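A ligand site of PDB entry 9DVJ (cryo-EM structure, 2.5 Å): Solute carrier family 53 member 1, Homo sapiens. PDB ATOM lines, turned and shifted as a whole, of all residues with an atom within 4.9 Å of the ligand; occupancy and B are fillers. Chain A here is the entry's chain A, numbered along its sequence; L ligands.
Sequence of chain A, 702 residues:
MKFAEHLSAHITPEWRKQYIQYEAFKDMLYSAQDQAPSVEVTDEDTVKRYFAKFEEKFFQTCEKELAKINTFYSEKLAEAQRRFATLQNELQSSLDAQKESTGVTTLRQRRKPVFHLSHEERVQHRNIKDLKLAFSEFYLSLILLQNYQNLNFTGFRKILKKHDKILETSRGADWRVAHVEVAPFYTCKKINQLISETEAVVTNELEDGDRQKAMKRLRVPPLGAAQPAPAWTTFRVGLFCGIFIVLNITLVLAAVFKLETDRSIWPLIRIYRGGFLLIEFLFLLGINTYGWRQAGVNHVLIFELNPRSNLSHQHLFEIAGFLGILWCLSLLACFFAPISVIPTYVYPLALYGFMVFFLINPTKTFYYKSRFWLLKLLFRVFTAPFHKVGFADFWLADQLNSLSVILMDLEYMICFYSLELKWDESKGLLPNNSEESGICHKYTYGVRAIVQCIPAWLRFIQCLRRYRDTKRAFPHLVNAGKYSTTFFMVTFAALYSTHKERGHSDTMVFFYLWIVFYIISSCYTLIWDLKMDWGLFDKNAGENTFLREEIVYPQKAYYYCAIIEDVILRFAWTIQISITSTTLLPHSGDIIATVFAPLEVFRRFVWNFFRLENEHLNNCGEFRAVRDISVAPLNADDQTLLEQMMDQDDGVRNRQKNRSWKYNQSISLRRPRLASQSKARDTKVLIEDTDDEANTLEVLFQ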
ATOM      1  N   LEU A 278      -0.311  -6.031  16.098  1.00  0.00           N
ATOM      2  CA  LEU A 278      -1.565  -5.293  16.236  1.00  0.00           C
ATOM      3  C   LEU A 278      -1.541  -4.368  17.440  1.00  0.00           C
ATOM      4  O   LEU A 278      -1.982  -3.211  17.354  1.00  0.00           O
ATOM      5  CB  LEU A 278      -2.729  -6.285  16.338  1.00  0.00           C
ATOM      6  CG  LEU A 278      -4.130  -5.686  16.419  1.00  0.00           C
ATOM      7  CD1 LEU A 278      -4.684  -5.424  15.026  1.00  0.00           C
ATOM      8  CD2 LEU A 278      -5.060  -6.600  17.195  1.00  0.00           C
ATOM      9  N   PHE A 281       0.697  -1.459  16.675  1.00  0.00           N
ATOM     10  CA  PHE A 281       0.028  -0.556  15.745  1.00  0.00           C
ATOM     11  C   PHE A 281      -1.011   0.299  16.461  1.00  0.00           C
ATOM     12  O   PHE A 281      -1.144   1.491  16.183  1.00  0.00           O
ATOM     13  CB  PHE A 281      -0.619  -1.341  14.609  1.00  0.00           C
ATOM     14  CG  PHE A 281      -1.439  -0.487  13.686  1.00  0.00           C
ATOM     15  CD1 PHE A 281      -0.841   0.490  12.912  1.00  0.00           C
ATOM     16  CD2 PHE A 281      -2.817  -0.664  13.585  1.00  0.00           C
ATOM     17  CE1 PHE A 281      -1.585   1.273  12.052  1.00  0.00           C
ATOM     18  CE2 PHE A 281      -3.563   0.120  12.735  1.00  0.00           C
ATOM     19  CZ  PHE A 281      -2.958   1.091  11.972  1.00  0.00           C
ATOM     20  N   LEU A 282      -1.765  -0.300  17.398  1.00  0.00           N
ATOM     21  CA  LEU A 282      -2.745   0.473  18.145  1.00  0.00           C
ATOM     22  C   LEU A 282      -2.064   1.562  18.984  1.00  0.00           C
ATOM     23  O   LEU A 282      -2.529   2.710  19.017  1.00  0.00           O
ATOM     24  CB  LEU A 282      -3.562  -0.453  19.045  1.00  0.00           C
ATOM     25  CG  LEU A 282      -4.575  -1.370  18.343  1.00  0.00           C
ATOM     26  CD1 LEU A 282      -5.307  -2.225  19.357  1.00  0.00           C
ATOM     27  CD2 LEU A 282      -5.570  -0.562  17.515  1.00  0.00           C
ATOM     28  N   LEU A 285      -0.875   4.255  16.735  1.00  0.00           N
ATOM     29  CA  LEU A 285      -1.994   5.027  16.219  1.00  0.00           C
ATOM     30  C   LEU A 285      -2.501   6.016  17.254  1.00  0.00           C
ATOM     31  O   LEU A 285      -2.878   7.140  16.915  1.00  0.00           O
ATOM     32  CB  LEU A 285      -3.122   4.079  15.789  1.00  0.00           C
ATOM     33  CG  LEU A 285      -4.190   4.669  14.867  1.00  0.00           C
ATOM     34  CD1 LEU A 285      -3.587   5.236  13.595  1.00  0.00           C
ATOM     35  CD2 LEU A 285      -5.226   3.613  14.544  1.00  0.00           C
ATOM     36  N   THR A 289      -2.622  10.013  16.754  1.00  0.00           N
ATOM     37  CA  THR A 289      -3.759  10.886  17.036  1.00  0.00           C
ATOM     38  C   THR A 289      -3.360  12.035  17.953  1.00  0.00           C
ATOM     39  O   THR A 289      -3.743  13.188  17.721  1.00  0.00           O
ATOM     40  CB  THR A 289      -4.904  10.072  17.653  1.00  0.00           C
ATOM     41  OG1 THR A 289      -5.236   8.973  16.790  1.00  0.00           O
ATOM     42  CG2 THR A 289      -6.140  10.946  17.845  1.00  0.00           C
ATOM     43  N   TRP A 292      -1.310  14.504  15.897  1.00  0.00           N
ATOM     44  CA  TRP A 292      -2.159  15.255  14.987  1.00  0.00           C
ATOM     45  C   TRP A 292      -2.919  16.338  15.739  1.00  0.00           C
ATOM     46  O   TRP A 292      -3.026  17.475  15.265  1.00  0.00           O
ATOM     47  CB  TRP A 292      -3.141  14.328  14.279  1.00  0.00           C
ATOM     48  CG  TRP A 292      -2.500  13.324  13.369  1.00  0.00           C
ATOM     49  CD1 TRP A 292      -1.329  13.469  12.675  1.00  0.00           C
ATOM     50  CD2 TRP A 292      -2.997  12.027  13.035  1.00  0.00           C
ATOM     51  NE1 TRP A 292      -1.067  12.347  11.935  1.00  0.00           N
ATOM     52  CE2 TRP A 292      -2.073  11.435  12.140  1.00  0.00           C
ATOM     53  CE3 TRP A 292      -4.131  11.296  13.407  1.00  0.00           C
ATOM     54  CZ2 TRP A 292      -2.254  10.154  11.626  1.00  0.00           C
ATOM     55  CZ3 TRP A 292      -4.306  10.023  12.893  1.00  0.00           C
ATOM     56  CH2 TRP A 292      -3.367   9.470  12.007  1.00  0.00           C
ATOM     57  N   HIS A 299      -7.161  15.924  11.268  1.00  0.00           N
ATOM     58  CA  HIS A 299      -7.318  14.510  10.937  1.00  0.00           C
ATOM     59  C   HIS A 299      -8.788  14.099  10.951  1.00  0.00           C
ATOM     60  O   HIS A 299      -9.190  13.213  10.189  1.00  0.00           O
ATOM     61  CB  HIS A 299      -6.508  13.650  11.899  1.00  0.00           C
ATOM     62  CG  HIS A 299      -7.180  13.422  13.224  1.00  0.00           C
ATOM     63  ND1 HIS A 299      -8.109  12.428  13.431  1.00  0.00           N
ATOM     64  CD2 HIS A 299      -7.040  14.061  14.407  1.00  0.00           C
ATOM     65  CE1 HIS A 299      -8.520  12.466  14.686  1.00  0.00           C
ATOM     66  NE2 HIS A 299      -7.888  13.445  15.295  1.00  0.00           N
ATOM     67  N   PHE A 303     -10.316  12.384   7.657  1.00  0.00           N
ATOM     68  CA  PHE A 303     -10.937  11.073   7.744  1.00  0.00           C
ATOM     69  C   PHE A 303     -12.465  11.132   7.644  1.00  0.00           C
ATOM     70  O   PHE A 303     -13.100  10.084   7.633  1.00  0.00           O
ATOM     71  CB  PHE A 303     -10.542  10.382   9.046  1.00  0.00           C
ATOM     72  CG  PHE A 303      -9.181   9.737   9.005  1.00  0.00           C
ATOM     73  CD1 PHE A 303      -8.952   8.615   8.231  1.00  0.00           C
ATOM     74  CD2 PHE A 303      -8.142  10.247   9.755  1.00  0.00           C
ATOM     75  CE1 PHE A 303      -7.706   8.019   8.195  1.00  0.00           C
ATOM     76  CE2 PHE A 303      -6.891   9.659   9.729  1.00  0.00           C
ATOM     77  CZ  PHE A 303      -6.676   8.549   8.943  1.00  0.00           C
ATOM     78  N   LEU A 305     -14.560  11.993   9.893  1.00  0.00           N
ATOM     79  CA  LEU A 305     -15.091  11.447  11.121  1.00  0.00           C
ATOM     80  C   LEU A 305     -16.025  12.449  11.789  1.00  0.00           C
ATOM     81  O   LEU A 305     -15.937  13.661  11.562  1.00  0.00           O
ATOM     82  CB  LEU A 305     -13.962  11.061  12.077  1.00  0.00           C
ATOM     83  CG  LEU A 305     -13.055   9.939  11.575  1.00  0.00           C
ATOM     84  CD1 LEU A 305     -11.665  10.050  12.194  1.00  0.00           C
ATOM     85  CD2 LEU A 305     -13.655   8.573  11.839  1.00  0.00           C
ATOM     86  N   ASN A 306     -16.920  11.945  12.624  1.00  0.00           N
ATOM     87  CA  ASN A 306     -17.903  12.796  13.286  1.00  0.00           C
ATOM     88  C   ASN A 306     -17.192  13.748  14.247  1.00  0.00           C
ATOM     89  O   ASN A 306     -16.455  13.295  15.127  1.00  0.00           O
ATOM     90  CB  ASN A 306     -18.927  11.952  14.038  1.00  0.00           C
ATOM     91  CG  ASN A 306     -20.118  12.775  14.510  1.00  0.00           C
ATOM     92  OD1 ASN A 306     -19.976  13.693  15.314  1.00  0.00           O
ATOM     93  ND2 ASN A 306     -21.297  12.430  14.007  1.00  0.00           N
ATOM     94  N   SER A 309     -18.397  13.203  18.216  1.00  0.00           N
ATOM     95  CA  SER A 309     -17.904  11.986  18.835  1.00  0.00           C
ATOM     96  C   SER A 309     -16.563  11.603  18.221  1.00  0.00           C
ATOM     97  O   SER A 309     -16.456  11.454  17.003  1.00  0.00           O
ATOM     98  CB  SER A 309     -18.914  10.846  18.671  1.00  0.00           C
ATOM     99  OG  SER A 309     -19.072  10.498  17.306  1.00  0.00           O
ATOM    100  N   ASN A 310     -15.551  11.443  19.071  1.00  0.00           N
ATOM    101  CA  ASN A 310     -14.211  11.109  18.625  1.00  0.00           C
ATOM    102  C   ASN A 310     -13.571  10.164  19.625  1.00  0.00           C
ATOM    103  O   ASN A 310     -13.901  10.180  20.819  1.00  0.00           O
ATOM    104  CB  ASN A 310     -13.340  12.370  18.466  1.00  0.00           C
ATOM    105  CG  ASN A 310     -13.566  13.061  17.131  1.00  0.00           C
ATOM    106  OD1 ASN A 310     -14.096  12.472  16.196  1.00  0.00           O
ATOM    107  ND2 ASN A 310     -13.147  14.322  17.046  1.00  0.00           N
ATOM    108  N   LEU A 311     -12.652   9.345  19.136  1.00  0.00           N
ATOM    109  CA  LEU A 311     -11.888   8.434  19.976  1.00  0.00           C
ATOM    110  C   LEU A 311     -10.578   9.096  20.362  1.00  0.00           C
ATOM    111  O   LEU A 311      -9.714   9.337  19.499  1.00  0.00           O
ATOM    112  CB  LEU A 311     -11.633   7.105  19.258  1.00  0.00           C
ATOM    113  CG  LEU A 311     -11.031   6.002  20.134  1.00  0.00           C
ATOM    114  CD1 LEU A 311     -12.097   5.400  21.038  1.00  0.00           C
ATOM    115  CD2 LEU A 311     -10.372   4.934  19.290  1.00  0.00           C
ATOM    116  N   LEU A 316      -7.354   4.744  22.675  1.00  0.00           N
ATOM    117  CA  LEU A 316      -6.531   3.827  21.910  1.00  0.00           C
ATOM    118  C   LEU A 316      -5.453   3.206  22.784  1.00  0.00           C
ATOM    119  O   LEU A 316      -5.174   1.998  22.686  1.00  0.00           O
ATOM    120  CB  LEU A 316      -5.900   4.547  20.722  1.00  0.00           C
ATOM    121  CG  LEU A 316      -6.820   4.830  19.532  1.00  0.00           C
ATOM    122  CD1 LEU A 316      -6.186   5.820  18.579  1.00  0.00           C
ATOM    123  CD2 LEU A 316      -7.180   3.537  18.809  1.00  0.00           C
ATOM    124  N   ILE A 319      -7.130   0.530  24.932  1.00  0.00           N
ATOM    125  CA  ILE A 319      -7.419  -0.679  24.161  1.00  0.00           C
ATOM    126  C   ILE A 319      -6.141  -1.471  23.929  1.00  0.00           C
ATOM    127  O   ILE A 319      -6.105  -2.699  24.089  1.00  0.00           O
ATOM    128  CB  ILE A 319      -8.115  -0.324  22.839  1.00  0.00           C
ATOM    129  CG1 ILE A 319      -9.431   0.421  23.090  1.00  0.00           C
ATOM    130  CG2 ILE A 319      -8.370  -1.582  22.014  1.00  0.00           C
ATOM    131  CD1 ILE A 319      -9.805   1.381  21.985  1.00  0.00           C
ATOM    132  N   LEU A 323      -5.359  -5.265  25.331  1.00  0.00           N
ATOM    133  CA  LEU A 323      -5.035  -6.343  24.393  1.00  0.00           C
ATOM    134  C   LEU A 323      -3.645  -6.902  24.672  1.00  0.00           C
ATOM    135  O   LEU A 323      -3.438  -8.118  24.597  1.00  0.00           O
ATOM    136  CB  LEU A 323      -5.140  -5.830  22.961  1.00  0.00           C
ATOM    137  CG  LEU A 323      -6.543  -5.558  22.417  1.00  0.00           C
ATOM    138  CD1 LEU A 323      -6.489  -5.225  20.942  1.00  0.00           C
ATOM    139  CD2 LEU A 323      -7.478  -6.735  22.665  1.00  0.00           C
ATOM    140  N   MET A 355     -10.238 -11.222  20.674  1.00  0.00           N
ATOM    141  CA  MET A 355      -9.959  -9.995  19.922  1.00  0.00           C
ATOM    142  C   MET A 355     -10.972  -9.805  18.799  1.00  0.00           C
ATOM    143  O   MET A 355     -11.539  -8.716  18.633  1.00  0.00           O
ATOM    144  CB  MET A 355      -8.536 -10.040  19.356  1.00  0.00           C
ATOM    145  CG  MET A 355      -7.435  -9.994  20.403  1.00  0.00           C
ATOM    146  SD  MET A 355      -5.794  -9.950  19.673  1.00  0.00           S
ATOM    147  CE  MET A 355      -4.851  -9.190  20.982  1.00  0.00           C
ATOM    148  N   VAL A 356     -11.225 -10.866  18.022  1.00  0.00           N
ATOM    149  CA  VAL A 356     -12.163 -10.759  16.912  1.00  0.00           C
ATOM    150  C   VAL A 356     -13.557 -10.434  17.413  1.00  0.00           C
ATOM    151  O   VAL A 356     -14.253  -9.578  16.855  1.00  0.00           O
ATOM    152  CB  VAL A 356     -12.146 -12.058  16.077  1.00  0.00           C
ATOM    153  CG1 VAL A 356     -13.335 -12.102  15.132  1.00  0.00           C
ATOM    154  CG2 VAL A 356     -10.845 -12.159  15.291  1.00  0.00           C
ATOM    155  N   PHE A 358     -14.392  -8.914  20.194  1.00  0.00           N
ATOM    156  CA  PHE A 358     -14.400  -7.528  20.652  1.00  0.00           C
ATOM    157  C   PHE A 358     -14.530  -6.575  19.482  1.00  0.00           C
ATOM    158  O   PHE A 358     -15.275  -5.592  19.546  1.00  0.00           O
ATOM    159  CB  PHE A 358     -13.124  -7.247  21.451  1.00  0.00           C
ATOM    160  CG  PHE A 358     -12.939  -5.791  21.803  1.00  0.00           C
ATOM    161  CD1 PHE A 358     -12.329  -4.922  20.916  1.00  0.00           C
ATOM    162  CD2 PHE A 358     -13.362  -5.305  23.029  1.00  0.00           C
ATOM    163  CE1 PHE A 358     -12.154  -3.584  21.244  1.00  0.00           C
ATOM    164  CE2 PHE A 358     -13.192  -3.975  23.357  1.00  0.00           C
ATOM    165  CZ  PHE A 358     -12.588  -3.115  22.460  1.00  0.00           C
ATOM    166  N   LEU A 359     -13.799  -6.843  18.385  1.00  0.00           N
ATOM    167  CA  LEU A 359     -13.914  -5.989  17.213  1.00  0.00           C
ATOM    168  C   LEU A 359     -15.323  -6.036  16.627  1.00  0.00           C
ATOM    169  O   LEU A 359     -15.867  -4.997  16.215  1.00  0.00           O
ATOM    170  CB  LEU A 359     -12.885  -6.406  16.156  1.00  0.00           C
ATOM    171  CG  LEU A 359     -12.953  -5.635  14.832  1.00  0.00           C
ATOM    172  CD1 LEU A 359     -12.827  -4.133  15.055  1.00  0.00           C
ATOM    173  CD2 LEU A 359     -11.872  -6.131  13.876  1.00  0.00           C
ATOM    174  N   LYS A 369     -19.531   2.628  18.308  1.00  0.00           N
ATOM    175  CA  LYS A 369     -19.647   3.422  17.089  1.00  0.00           C
ATOM    176  C   LYS A 369     -18.356   3.353  16.280  1.00  0.00           C
ATOM    177  O   LYS A 369     -18.381   3.128  15.062  1.00  0.00           O
ATOM    178  CB  LYS A 369     -19.984   4.868  17.428  1.00  0.00           C
ATOM    179  CG  LYS A 369     -21.218   5.042  18.298  1.00  0.00           C
ATOM    180  CD  LYS A 369     -21.545   6.509  18.506  1.00  0.00           C
ATOM    181  CE  LYS A 369     -22.580   6.706  19.596  1.00  0.00           C
ATOM    182  NZ  LYS A 369     -22.917   8.142  19.805  1.00  0.00           N
ATOM    183  N   SER A 370     -17.218   3.540  16.939  1.00  0.00           N
ATOM    184  CA  SER A 370     -15.933   3.500  16.238  1.00  0.00           C
ATOM    185  C   SER A 370     -15.663   2.107  15.687  1.00  0.00           C
ATOM    186  O   SER A 370     -15.123   1.969  14.583  1.00  0.00           O
ATOM    187  CB  SER A 370     -14.815   3.935  17.182  1.00  0.00           C
ATOM    188  OG  SER A 370     -14.954   3.332  18.454  1.00  0.00           O
ATOM    189  N   ARG A 371     -16.027   1.068  16.439  1.00  0.00           N
ATOM    190  CA  ARG A 371     -15.819  -0.293  15.950  1.00  0.00           C
ATOM    191  C   ARG A 371     -16.661  -0.555  14.701  1.00  0.00           C
ATOM    192  O   ARG A 371     -16.185  -1.184  13.751  1.00  0.00           O
ATOM    193  CB  ARG A 371     -16.157  -1.294  17.055  1.00  0.00           C
ATOM    194  CG  ARG A 371     -15.091  -1.409  18.118  1.00  0.00           C
ATOM    195  CD  ARG A 371     -15.383  -2.543  19.085  1.00  0.00           C
ATOM    196  NE  ARG A 371     -16.678  -2.394  19.728  1.00  0.00           N
ATOM    197  CZ  ARG A 371     -17.785  -3.021  19.350  1.00  0.00           C
ATOM    198  NH1 ARG A 371     -17.805  -3.840  18.311  1.00  0.00           N
ATOM    199  NH2 ARG A 371     -18.919  -2.819  20.027  1.00  0.00           N
ATOM    200  N   TRP A 373     -17.711   1.728  12.559  1.00  0.00           N
ATOM    201  CA  TRP A 373     -17.111   2.495  11.475  1.00  0.00           C
ATOM    202  C   TRP A 373     -15.884   1.771  10.921  1.00  0.00           C
ATOM    203  O   TRP A 373     -15.683   1.714   9.706  1.00  0.00           O
ATOM    204  CB  TRP A 373     -16.737   3.894  11.961  1.00  0.00           C
ATOM    205  CG  TRP A 373     -16.002   4.721  10.948  1.00  0.00           C
ATOM    206  CD1 TRP A 373     -16.550   5.608  10.062  1.00  0.00           C
ATOM    207  CD2 TRP A 373     -14.593   4.756  10.719  1.00  0.00           C
ATOM    208  NE1 TRP A 373     -15.565   6.182   9.302  1.00  0.00           N
ATOM    209  CE2 TRP A 373     -14.351   5.678   9.690  1.00  0.00           C
ATOM    210  CE3 TRP A 373     -13.502   4.092  11.295  1.00  0.00           C
ATOM    211  CZ2 TRP A 373     -13.076   5.955   9.210  1.00  0.00           C
ATOM    212  CZ3 TRP A 373     -12.233   4.361  10.815  1.00  0.00           C
ATOM    213  CH2 TRP A 373     -12.027   5.285   9.782  1.00  0.00           C
ATOM    214  N   LEU A 374     -15.061   1.216  11.806  1.00  0.00           N
ATOM    215  CA  LEU A 374     -13.879   0.487  11.358  1.00  0.00           C
ATOM    216  C   LEU A 374     -14.269  -0.759  10.569  1.00  0.00           C
ATOM    217  O   LEU A 374     -13.624  -1.089   9.568  1.00  0.00           O
ATOM    218  CB  LEU A 374     -13.011   0.105  12.569  1.00  0.00           C
ATOM    219  CG  LEU A 374     -11.976  -1.005  12.371  1.00  0.00           C
ATOM    220  CD1 LEU A 374     -10.996  -0.623  11.270  1.00  0.00           C
ATOM    221  CD2 LEU A 374     -11.247  -1.284  13.672  1.00  0.00           C
ATOM    222  N   LEU A 378     -13.197  -1.465   6.754  1.00  0.00           N
ATOM    223  CA  LEU A 378     -12.500  -2.668   6.326  1.00  0.00           C
ATOM    224  C   LEU A 378     -13.254  -3.374   5.204  1.00  0.00           C
ATOM    225  O   LEU A 378     -12.652  -3.809   4.216  1.00  0.00           O
ATOM    226  CB  LEU A 378     -12.322  -3.620   7.511  1.00  0.00           C
ATOM    227  CG  LEU A 378     -11.340  -3.186   8.603  1.00  0.00           C
ATOM    228  CD1 LEU A 378     -11.771  -3.708   9.960  1.00  0.00           C
ATOM    229  CD2 LEU A 378      -9.932  -3.661   8.263  1.00  0.00           C
ATOM    230  N   TRP A 395      -5.929   4.950   3.370  1.00  0.00           N
ATOM    231  CA  TRP A 395      -5.087   4.914   4.557  1.00  0.00           C
ATOM    232  C   TRP A 395      -5.112   3.535   5.204  1.00  0.00           C
ATOM    233  O   TRP A 395      -4.069   2.985   5.577  1.00  0.00           O
ATOM    234  CB  TRP A 395      -5.552   5.984   5.551  1.00  0.00           C
ATOM    235  CG  TRP A 395      -4.768   6.039   6.817  1.00  0.00           C
ATOM    236  CD1 TRP A 395      -3.715   6.858   7.096  1.00  0.00           C
ATOM    237  CD2 TRP A 395      -4.988   5.261   8.000  1.00  0.00           C
ATOM    238  NE1 TRP A 395      -3.256   6.631   8.366  1.00  0.00           N
ATOM    239  CE2 TRP A 395      -4.023   5.660   8.951  1.00  0.00           C
ATOM    240  CE3 TRP A 395      -5.901   4.265   8.341  1.00  0.00           C
ATOM    241  CZ2 TRP A 395      -3.950   5.086  10.213  1.00  0.00           C
ATOM    242  CZ3 TRP A 395      -5.822   3.699   9.602  1.00  0.00           C
ATOM    243  CH2 TRP A 395      -4.856   4.110  10.522  1.00  0.00           C
ATOM    244  N   LEU A 396      -6.307   2.941   5.329  1.00  0.00           N
ATOM    245  CA  LEU A 396      -6.403   1.604   5.905  1.00  0.00           C
ATOM    246  C   LEU A 396      -5.730   0.564   5.021  1.00  0.00           C
ATOM    247  O   LEU A 396      -5.116  -0.379   5.525  1.00  0.00           O
ATOM    248  CB  LEU A 396      -7.879   1.245   6.128  1.00  0.00           C
ATOM    249  CG  LEU A 396      -8.130  -0.017   6.945  1.00  0.00           C
ATOM    250  CD1 LEU A 396      -7.995   0.259   8.443  1.00  0.00           C
ATOM    251  CD2 LEU A 396      -9.501  -0.596   6.628  1.00  0.00           C
ATOM    252  N   ILE A 406       0.805 -10.225   9.371  1.00  0.00           N
ATOM    253  CA  ILE A 406      -0.269 -10.930  10.060  1.00  0.00           C
ATOM    254  C   ILE A 406      -0.924 -11.938   9.118  1.00  0.00           C
ATOM    255  O   ILE A 406      -1.164 -13.088   9.486  1.00  0.00           O
ATOM    256  CB  ILE A 406      -1.301  -9.929  10.617  1.00  0.00           C
ATOM    257  CG1 ILE A 406      -0.611  -8.821  11.405  1.00  0.00           C
ATOM    258  CG2 ILE A 406      -2.302 -10.667  11.496  1.00  0.00           C
ATOM    259  CD1 ILE A 406      -1.554  -7.760  11.927  1.00  0.00           C
HETATM  260  C1  LIG L   1     -12.302   8.699  15.647  1.00  0.00           C
HETATM  261  C2  LIG L   1     -10.939   7.994  15.377  1.00  0.00           C
HETATM  262  C3  LIG L   1     -11.234   6.690  14.581  1.00  0.00           C
HETATM  263  C4  LIG L   1     -15.740   7.136  14.261  1.00  0.00           C
HETATM  264  C5  LIG L   1     -17.096   6.670  14.754  1.00  0.00           C
HETATM  265  C6  LIG L   1     -18.004   7.757  12.640  1.00  0.00           C
HETATM  266  C7  LIG L   1     -18.006   8.913  14.844  1.00  0.00           C
HETATM  267  C8  LIG L   1     -19.563   7.048  14.447  1.00  0.00           C
HETATM  268  C9  LIG L   1     -12.005   4.475  15.001  1.00  0.00           C
HETATM  269  C10 LIG L   1     -11.560   3.353  15.912  1.00  0.00           C
HETATM  270  C11 LIG L   1     -10.064   3.046  15.742  1.00  0.00           C
HETATM  271  C12 LIG L   1      -9.661   1.661  16.272  1.00  0.00           C
HETATM  272  C13 LIG L   1     -10.089   1.397  17.725  1.00  0.00           C
HETATM  273  C14 LIG L   1      -9.797  -0.053  18.177  1.00  0.00           C
HETATM  274  C15 LIG L   1     -10.951  -1.047  17.948  1.00  0.00           C
HETATM  275  C16 LIG L   1     -10.571  -2.511  18.239  1.00  0.00           C
HETATM  276  C17 LIG L   1      -9.605  -3.170  17.231  1.00  0.00           C
HETATM  277  C18 LIG L   1      -9.244  -4.656  17.450  1.00  0.00           C
HETATM  278  C19 LIG L   1      -8.648  -5.409  16.259  1.00  0.00           C
HETATM  279  C20 LIG L   1      -8.783  -6.935  16.399  1.00  0.00           C
HETATM  280  C21 LIG L   1      -8.245  -7.745  15.216  1.00  0.00           C
HETATM  281  C22 LIG L   1      -8.159  -9.251  15.489  1.00  0.00           C
HETATM  282  C23 LIG L   1      -7.354  -9.987  14.408  1.00  0.00           C
HETATM  283  C24 LIG L   1      -8.071  -9.917  13.071  1.00  0.00           C
HETATM  284  C25 LIG L   1      -8.764   8.479  14.393  1.00  0.00           C
HETATM  285  C26 LIG L   1      -8.276   8.573  12.947  1.00  0.00           C
HETATM  286  C27 LIG L   1      -8.769   7.381  12.103  1.00  0.00           C
HETATM  287  C28 LIG L   1      -8.038   6.078  12.460  1.00  0.00           C
HETATM  288  C29 LIG L   1      -8.817   4.817  12.085  1.00  0.00           C
HETATM  289  C30 LIG L   1      -8.077   3.532  12.472  1.00  0.00           C
HETATM  290  C31 LIG L   1      -8.764   2.242  12.018  1.00  0.00           C
HETATM  291  C32 LIG L   1      -7.853   1.008  12.107  1.00  0.00           C
HETATM  292  C33 LIG L   1      -7.609   0.628  13.536  1.00  0.00           C
HETATM  293  C34 LIG L   1      -7.599  -0.600  14.036  1.00  0.00           C
HETATM  294  C35 LIG L   1      -7.860  -1.854  13.270  1.00  0.00           C
HETATM  295  C36 LIG L   1      -6.637  -2.297  12.547  1.00  0.00           C
HETATM  296  C37 LIG L   1      -6.543  -3.381  11.778  1.00  0.00           C
HETATM  297  C38 LIG L   1      -7.663  -4.337  11.510  1.00  0.00           C
HETATM  298  C39 LIG L   1      -7.595  -5.601  12.371  1.00  0.00           C
HETATM  299  C40 LIG L   1      -6.370  -6.451  12.035  1.00  0.00           C
HETATM  300  C41 LIG L   1      -6.428  -6.998  10.603  1.00  0.00           C
HETATM  301  C42 LIG L   1      -5.473  -8.161  10.420  1.00  0.00           C
HETATM  302  N1  LIG L   1     -18.170   7.584  14.144  1.00  0.00           N
HETATM  303  O1  LIG L   1     -10.052   8.841  14.631  1.00  0.00           O
HETATM  304  O2  LIG L   1     -11.751   5.727  15.474  1.00  0.00           O
HETATM  305  O3  LIG L   1     -12.548   4.311  13.938  1.00  0.00           O
HETATM  306  O4  LIG L   1      -8.003   8.108  15.270  1.00  0.00           O
HETATM  307  O5  LIG L   1     -15.127   7.272  17.760  1.00  0.00           O
HETATM  308  O6  LIG L   1     -15.057   9.359  15.987  1.00  0.00           O
HETATM  309  O7  LIG L   1     -13.030   7.895  16.477  1.00  0.00           O
HETATM  310  O8  LIG L   1     -14.845   6.849  15.267  1.00  0.00           O
HETATM  311  P1  LIG L   1     -14.766   8.008  16.523  1.00  0.00           P
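N of Ser 309 sits at hydrogen-bond distance from OD1 of Asn 306, at 3.3 Å.
The side-chain amide oxygen of Asn 310 sits close to the backbone carbonyl oxygen of Asn 306, at 2.7 Å.
The side-chain hydroxyl (OG1) of Thr 289 lies within hydrogen-bond range of the backbone carbonyl oxygen (O) of Leu 285 (3.0 Å).
The backbone carbonyl oxygen (O) of Phe 358 lies close to the guanidinium group (NH1) of Arg 371 (3.3 Å).
Residues that only touch the ligand: Trp 373, Leu 305, Asn 306, Ser 370, Leu 374, Leu 285, Phe 358, Leu 278, Phe 303, Trp 395, Lys 369, Leu 396, Leu 316, His 299, Phe 281, Val 356 and Met 355.
Hydrophobic or aromatic side chains within 4 Å of the ligand: Leu 278, Phe 281, Leu 285, His 299, Phe 303, Leu 305, Leu 311, Leu 316, Met 355, Val 356, Phe 358, Trp 373, Leu 374, Trp 395 and Leu 396.
21 residues have an atom within 4 Å of the ligand: Leu 278, Phe 281, Leu 285, Thr 289, His 299, Phe 303, Leu 305, Asn 306, Ser 309, Asn 310, Leu 311, Leu 316, Met 355, Val 356, Phe 358, Lys 369, Ser 370, Trp 373, Leu 374, Trp 395 and Leu 396.
The nearest printed residue that does not touch the ligand is Leu 359 (4.01 Å).
The backbone carbonyl oxygen (O) of Ser 309 sits close to an oxygen (O6) of the ligand.
O7 of the ligand lies within hydrogen-bond range of N of Leu 311, 3.1 Å away.
An oxygen (O6) of the ligand sits close to the side-chain amide oxygen (OD1) of Asn 310 (3.3 Å).
The side-chain hydroxyl (OG1) of Thr 289 lies within hydrogen-bond range of an oxygen (O4) of the ligand, 3.3 Å away.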
